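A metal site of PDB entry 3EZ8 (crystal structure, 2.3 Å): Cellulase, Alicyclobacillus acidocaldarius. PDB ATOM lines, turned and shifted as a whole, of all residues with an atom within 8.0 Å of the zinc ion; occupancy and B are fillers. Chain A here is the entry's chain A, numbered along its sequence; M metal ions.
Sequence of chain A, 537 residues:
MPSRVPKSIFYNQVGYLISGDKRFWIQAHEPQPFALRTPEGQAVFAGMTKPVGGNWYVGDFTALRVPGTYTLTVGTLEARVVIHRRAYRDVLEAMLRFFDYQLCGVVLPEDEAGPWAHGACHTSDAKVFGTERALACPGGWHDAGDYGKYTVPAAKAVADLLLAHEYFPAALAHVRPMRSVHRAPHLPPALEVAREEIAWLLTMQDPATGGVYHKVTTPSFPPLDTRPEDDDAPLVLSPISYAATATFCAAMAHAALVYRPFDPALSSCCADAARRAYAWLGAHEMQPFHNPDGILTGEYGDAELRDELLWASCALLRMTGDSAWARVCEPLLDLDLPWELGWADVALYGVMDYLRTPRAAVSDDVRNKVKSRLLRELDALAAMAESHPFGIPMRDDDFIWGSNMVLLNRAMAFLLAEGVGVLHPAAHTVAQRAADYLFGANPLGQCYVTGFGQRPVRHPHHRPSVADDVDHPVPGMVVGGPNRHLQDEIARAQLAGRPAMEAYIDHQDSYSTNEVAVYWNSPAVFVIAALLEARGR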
ATOM      1  N   GLN A 102       9.987 -32.056   1.801  1.00  0.00           N
ATOM      2  CA  GLN A 102       9.307 -30.807   2.115  1.00  0.00           C
ATOM      3  C   GLN A 102       8.000 -30.628   1.342  1.00  0.00           C
ATOM      4  O   GLN A 102       7.283 -29.647   1.569  1.00  0.00           O
ATOM      5  CB  GLN A 102      10.225 -29.606   1.842  1.00  0.00           C
ATOM      6  CG  GLN A 102      11.430 -29.509   2.762  1.00  0.00           C
ATOM      7  CD  GLN A 102      11.047 -29.205   4.199  1.00  0.00           C
ATOM      8  OE1 GLN A 102      11.016 -30.101   5.047  1.00  0.00           O
ATOM      9  NE2 GLN A 102      10.764 -27.936   4.479  1.00  0.00           N
ATOM     10  N   LEU A 103       7.703 -31.560   0.443  1.00  0.00           N
ATOM     11  CA  LEU A 103       6.526 -31.480  -0.413  1.00  0.00           C
ATOM     12  C   LEU A 103       5.202 -31.368   0.355  1.00  0.00           C
ATOM     13  O   LEU A 103       4.957 -32.108   1.300  1.00  0.00           O
ATOM     14  CB  LEU A 103       6.473 -32.673  -1.373  1.00  0.00           C
ATOM     15  CG  LEU A 103       7.323 -32.619  -2.653  1.00  0.00           C
ATOM     16  CD1 LEU A 103       7.360 -33.981  -3.315  1.00  0.00           C
ATOM     17  CD2 LEU A 103       6.792 -31.572  -3.624  1.00  0.00           C
ATOM     18  N   CYS A 104       4.382 -30.413  -0.088  1.00  0.00           N
ATOM     19  CA  CYS A 104       3.100 -30.133   0.537  1.00  0.00           C
ATOM     20  C   CYS A 104       1.956 -30.566  -0.375  1.00  0.00           C
ATOM     21  O   CYS A 104       2.046 -30.422  -1.594  1.00  0.00           O
ATOM     22  CB  CYS A 104       2.987 -28.633   0.835  1.00  0.00           C
ATOM     23  SG  CYS A 104       1.419 -28.126   1.578  1.00  0.00           S
ATOM     24  N   GLY A 105       0.890 -31.100   0.216  1.00  0.00           N
ATOM     25  CA  GLY A 105      -0.302 -31.501  -0.534  1.00  0.00           C
ATOM     26  C   GLY A 105      -0.126 -32.728  -1.405  1.00  0.00           C
ATOM     27  O   GLY A 105      -0.850 -32.915  -2.382  1.00  0.00           O
ATOM     28  N   VAL A 106       0.843 -33.582  -1.046  1.00  0.00           N
ATOM     29  CA  VAL A 106       1.122 -34.806  -1.793  1.00  0.00           C
ATOM     30  C   VAL A 106       1.566 -35.930  -0.860  1.00  0.00           C
ATOM     31  O   VAL A 106       2.378 -35.706   0.051  1.00  0.00           O
ATOM     32  CB  VAL A 106       2.130 -34.572  -2.962  1.00  0.00           C
ATOM     33  CG1 VAL A 106       3.487 -34.099  -2.447  1.00  0.00           C
ATOM     34  CG2 VAL A 106       2.277 -35.809  -3.830  1.00  0.00           C
ATOM     35  N   HIS A 118       4.460 -39.475   5.070  1.00  0.00           N
ATOM     36  CA  HIS A 118       3.214 -38.897   5.564  1.00  0.00           C
ATOM     37  C   HIS A 118       2.172 -38.643   4.467  1.00  0.00           C
ATOM     38  O   HIS A 118       2.472 -38.738   3.279  1.00  0.00           O
ATOM     39  CB  HIS A 118       3.496 -37.604   6.363  1.00  0.00           C
ATOM     40  CG  HIS A 118       3.923 -36.440   5.520  1.00  0.00           C
ATOM     41  ND1 HIS A 118       3.076 -35.826   4.620  1.00  0.00           N
ATOM     42  CD2 HIS A 118       5.100 -35.774   5.453  1.00  0.00           C
ATOM     43  CE1 HIS A 118       3.717 -34.834   4.029  1.00  0.00           C
ATOM     44  NE2 HIS A 118       4.945 -34.784   4.511  1.00  0.00           N
ATOM     45  N   GLY A 119       0.952 -38.330   4.893  1.00  0.00           N
ATOM     46  CA  GLY A 119      -0.151 -38.054   3.978  1.00  0.00           C
ATOM     47  C   GLY A 119      -0.153 -36.637   3.436  1.00  0.00           C
ATOM     48  O   GLY A 119       0.541 -35.757   3.952  1.00  0.00           O
ATOM     49  N   ALA A 120      -0.951 -36.420   2.386  1.00  0.00           N
ATOM     50  CA  ALA A 120      -1.080 -35.109   1.743  1.00  0.00           C
ATOM     51  C   ALA A 120      -1.609 -34.061   2.713  1.00  0.00           C
ATOM     52  O   ALA A 120      -2.741 -34.157   3.200  1.00  0.00           O
ATOM     53  CB  ALA A 120      -1.964 -35.213   0.509  1.00  0.00           C
ATOM     54  N   CYS A 121      -0.782 -33.063   2.990  1.00  0.00           N
ATOM     55  CA  CYS A 121      -1.090 -32.036   3.979  1.00  0.00           C
ATOM     56  C   CYS A 121      -1.499 -30.714   3.333  1.00  0.00           C
ATOM     57  O   CYS A 121      -1.174 -30.450   2.176  1.00  0.00           O
ATOM     58  CB  CYS A 121       0.115 -31.817   4.889  1.00  0.00           C
ATOM     59  SG  CYS A 121       1.643 -31.388   4.016  1.00  0.00           S
ATOM     60  N   HIS A 122      -2.206 -29.881   4.109  1.00  0.00           N
ATOM     61  CA  HIS A 122      -2.615 -28.534   3.679  1.00  0.00           C
ATOM     62  C   HIS A 122      -3.341 -28.536   2.328  1.00  0.00           C
ATOM     63  O   HIS A 122      -2.957 -27.814   1.401  1.00  0.00           O
ATOM     64  CB  HIS A 122      -1.392 -27.598   3.650  1.00  0.00           C
ATOM     65  CG  HIS A 122      -0.627 -27.549   4.938  1.00  0.00           C
ATOM     66  ND1 HIS A 122       0.427 -28.394   5.206  1.00  0.00           N
ATOM     67  CD2 HIS A 122      -0.762 -26.753   6.020  1.00  0.00           C
ATOM     68  CE1 HIS A 122       0.903 -28.131   6.404  1.00  0.00           C
ATOM     69  NE2 HIS A 122       0.199 -27.142   6.925  1.00  0.00           N
ATOM     70  N   THR A 123      -4.391 -29.354   2.235  1.00  0.00           N
ATOM     71  CA  THR A 123      -5.111 -29.580   0.976  1.00  0.00           C
ATOM     72  C   THR A 123      -6.269 -28.618   0.738  1.00  0.00           C
ATOM     73  O   THR A 123      -6.888 -28.629  -0.333  1.00  0.00           O
ATOM     74  CB  THR A 123      -5.615 -31.040   0.875  1.00  0.00           C
ATOM     75  OG1 THR A 123      -6.195 -31.436   2.116  1.00  0.00           O
ATOM     76  CG2 THR A 123      -4.466 -31.982   0.528  1.00  0.00           C
ATOM     77  N   GLY A 139       0.639 -28.171  -3.594  1.00  0.00           N
ATOM     78  CA  GLY A 139       1.980 -28.580  -4.026  1.00  0.00           C
ATOM     79  C   GLY A 139       3.077 -27.693  -3.472  1.00  0.00           C
ATOM     80  O   GLY A 139       2.881 -26.991  -2.470  1.00  0.00           O
ATOM     81  N   GLY A 140       4.230 -27.725  -4.133  1.00  0.00           N
ATOM     82  CA  GLY A 140       5.383 -26.919  -3.718  1.00  0.00           C
ATOM     83  C   GLY A 140       6.068 -27.464  -2.490  1.00  0.00           C
ATOM     84  O   GLY A 140       5.948 -28.654  -2.179  1.00  0.00           O
ATOM     85  N   TRP A 141       6.790 -26.589  -1.793  1.00  0.00           N
ATOM     86  CA  TRP A 141       7.559 -26.999  -0.622  1.00  0.00           C
ATOM     87  C   TRP A 141       7.169 -26.237   0.632  1.00  0.00           C
ATOM     88  O   TRP A 141       6.855 -25.039   0.575  1.00  0.00           O
ATOM     89  CB  TRP A 141       9.060 -26.811  -0.865  1.00  0.00           C
ATOM     90  CG  TRP A 141       9.590 -27.529  -2.074  1.00  0.00           C
ATOM     91  CD1 TRP A 141       9.228 -28.772  -2.511  1.00  0.00           C
ATOM     92  CD2 TRP A 141      10.597 -27.057  -2.976  1.00  0.00           C
ATOM     93  NE1 TRP A 141       9.942 -29.098  -3.635  1.00  0.00           N
ATOM     94  CE2 TRP A 141      10.791 -28.059  -3.945  1.00  0.00           C
ATOM     95  CE3 TRP A 141      11.351 -25.878  -3.059  1.00  0.00           C
ATOM     96  CZ2 TRP A 141      11.707 -27.934  -4.997  1.00  0.00           C
ATOM     97  CZ3 TRP A 141      12.260 -25.750  -4.105  1.00  0.00           C
ATOM     98  CH2 TRP A 141      12.424 -26.764  -5.056  1.00  0.00           C
ATOM     99  N   HIS A 142       7.206 -26.930   1.772  1.00  0.00           N
ATOM    100  CA  HIS A 142       7.234 -26.267   3.069  1.00  0.00           C
ATOM    101  C   HIS A 142       8.565 -25.519   3.109  1.00  0.00           C
ATOM    102  O   HIS A 142       9.619 -26.118   2.881  1.00  0.00           O
ATOM    103  CB  HIS A 142       7.165 -27.288   4.215  1.00  0.00           C
ATOM    104  CG  HIS A 142       5.904 -28.098   4.239  1.00  0.00           C
ATOM    105  ND1 HIS A 142       5.907 -29.470   4.379  1.00  0.00           N
ATOM    106  CD2 HIS A 142       4.608 -27.734   4.150  1.00  0.00           C
ATOM    107  CE1 HIS A 142       4.670 -29.912   4.371  1.00  0.00           C
ATOM    108  NE2 HIS A 142       3.853 -28.881   4.236  1.00  0.00           N
ATOM    109  N   ASP A 146       8.801 -24.628   9.329  1.00  0.00           N
ATOM    110  CA  ASP A 146       7.345 -24.508   9.358  1.00  0.00           C
ATOM    111  C   ASP A 146       6.715 -25.078   8.080  1.00  0.00           C
ATOM    112  O   ASP A 146       7.358 -25.823   7.343  1.00  0.00           O
ATOM    113  CB  ASP A 146       6.930 -23.052   9.574  1.00  0.00           C
ATOM    114  CG  ASP A 146       7.302 -22.138   8.409  1.00  0.00           C
ATOM    115  OD1 ASP A 146       8.243 -22.470   7.648  1.00  0.00           O
ATOM    116  OD2 ASP A 146       6.660 -21.081   8.257  1.00  0.00           O
ATOM    117  N   TYR A 147       5.453 -24.720   7.850  1.00  0.00           N
ATOM    118  CA  TYR A 147       4.700 -25.222   6.703  1.00  0.00           C
ATOM    119  C   TYR A 147       4.248 -24.115   5.767  1.00  0.00           C
ATOM    120  O   TYR A 147       3.436 -24.339   4.857  1.00  0.00           O
ATOM    121  CB  TYR A 147       3.504 -26.047   7.188  1.00  0.00           C
ATOM    122  CG  TYR A 147       3.879 -27.250   8.029  1.00  0.00           C
ATOM    123  CD1 TYR A 147       4.828 -28.167   7.566  1.00  0.00           C
ATOM    124  CD2 TYR A 147       3.289 -27.477   9.265  1.00  0.00           C
ATOM    125  CE1 TYR A 147       5.170 -29.278   8.328  1.00  0.00           C
ATOM    126  CE2 TYR A 147       3.627 -28.577  10.034  1.00  0.00           C
ATOM    127  CZ  TYR A 147       4.569 -29.477   9.558  1.00  0.00           C
ATOM    128  OH  TYR A 147       4.909 -30.576  10.314  1.00  0.00           O
ATOM    129  N   GLY A 148       4.768 -22.909   5.979  1.00  0.00           N
ATOM    130  CA  GLY A 148       4.486 -21.776   5.112  1.00  0.00           C
ATOM    131  C   GLY A 148       5.120 -21.957   3.753  1.00  0.00           C
ATOM    132  O   GLY A 148       6.182 -22.563   3.625  1.00  0.00           O
ATOM    133  N   LYS A 149       4.452 -21.425   2.725  1.00  0.00           N
ATOM    134  CA  LYS A 149       4.978 -21.462   1.371  1.00  0.00           C
ATOM    135  C   LYS A 149       5.096 -20.034   0.848  1.00  0.00           C
ATOM    136  O   LYS A 149       4.113 -19.411   0.456  1.00  0.00           O
ATOM    137  CB  LYS A 149       4.079 -22.308   0.461  1.00  0.00           C
ATOM    138  CG  LYS A 149       3.894 -23.753   0.919  1.00  0.00           C
ATOM    139  CD  LYS A 149       3.244 -24.629  -0.150  1.00  0.00           C
ATOM    140  CE  LYS A 149       1.737 -24.407  -0.223  1.00  0.00           C
ATOM    141  NZ  LYS A 149       1.089 -25.383  -1.137  1.00  0.00           N
ATOM    142  N   PRO A 228       2.707 -32.667   9.687  1.00  0.00           N
ATOM    143  CA  PRO A 228       2.234 -31.915   8.527  1.00  0.00           C
ATOM    144  C   PRO A 228       0.712 -31.968   8.347  1.00  0.00           C
ATOM    145  O   PRO A 228       0.092 -30.946   8.065  1.00  0.00           O
ATOM    146  CB  PRO A 228       2.936 -32.591   7.353  1.00  0.00           C
ATOM    147  CG  PRO A 228       4.184 -33.136   7.940  1.00  0.00           C
ATOM    148  CD  PRO A 228       3.817 -33.578   9.318  1.00  0.00           C
ATOM    149  N   GLU A 229       0.134 -33.161   8.530  1.00  0.00           N
ATOM    150  CA  GLU A 229      -1.297 -33.365   8.286  1.00  0.00           C
ATOM    151  C   GLU A 229      -2.174 -33.273   9.550  1.00  0.00           C
ATOM    152  O   GLU A 229      -3.359 -33.635   9.512  1.00  0.00           O
ATOM    153  CB  GLU A 229      -1.544 -34.679   7.531  1.00  0.00           C
ATOM    154  CG  GLU A 229      -1.197 -35.957   8.290  1.00  0.00           C
ATOM    155  CD  GLU A 229       0.280 -36.308   8.283  1.00  0.00           C
ATOM    156  OE1 GLU A 229       1.090 -35.545   7.706  1.00  0.00           O
ATOM    157  OE2 GLU A 229       0.646 -37.349   8.854  1.00  0.00           O
ATOM    158  N   ASP A 231      -1.813 -30.221  10.947  1.00  0.00           N
ATOM    159  CA  ASP A 231      -1.914 -28.779  10.769  1.00  0.00           C
ATOM    160  C   ASP A 231      -3.133 -28.462   9.912  1.00  0.00           C
ATOM    161  O   ASP A 231      -3.061 -28.430   8.680  1.00  0.00           O
ATOM    162  CB  ASP A 231      -0.634 -28.221  10.129  1.00  0.00           C
ATOM    163  CG  ASP A 231      -0.531 -26.708  10.220  1.00  0.00           C
ATOM    164  OD1 ASP A 231      -1.224 -26.099  11.068  1.00  0.00           O
ATOM    165  OD2 ASP A 231       0.246 -26.111   9.452  1.00  0.00           O
ATOM    166  N   LEU A 235      -5.855 -21.670   5.596  1.00  0.00           N
ATOM    167  CA  LEU A 235      -4.792 -21.041   4.807  1.00  0.00           C
ATOM    168  C   LEU A 235      -5.262 -19.706   4.257  1.00  0.00           C
ATOM    169  O   LEU A 235      -6.407 -19.565   3.802  1.00  0.00           O
ATOM    170  CB  LEU A 235      -4.340 -21.966   3.671  1.00  0.00           C
ATOM    171  CG  LEU A 235      -3.683 -23.301   4.031  1.00  0.00           C
ATOM    172  CD1 LEU A 235      -3.661 -24.228   2.826  1.00  0.00           C
ATOM    173  CD2 LEU A 235      -2.272 -23.109   4.587  1.00  0.00           C
HETATM  174 ZN    ZN M   1       1.775 -29.060   3.536  1.00  0.00          ZN
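NE2 of His 122 is in hydrogen-bond range of OD2 of Asp 231, 2.7 Å away. The backbone carbonyl oxygen of Cys 104 lies close to the backbone NH of Gly 139, at 3.3 Å. The backbone carbonyl oxygen of Gly 140 sits at hydrogen-bond distance from the backbone NH of Cys 104 (3.1 Å). O of His 142 is in hydrogen-bond range of NE2 of Gln 102, at 2.7 Å. The backbone carbonyl oxygen of Cys 121 sits at hydrogen-bond distance from the backbone NH of Gly 105 (2.9 Å).
N of Gly 105 touches the zinc ion (3.996 Å).
The zinc ion is bound by SG of Cys 104 (2.2 Å), NE2 of His 142 (2.2 Å), ND1 of His 122 (2.2 Å) and SG of Cys 121 (2.4 Å).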
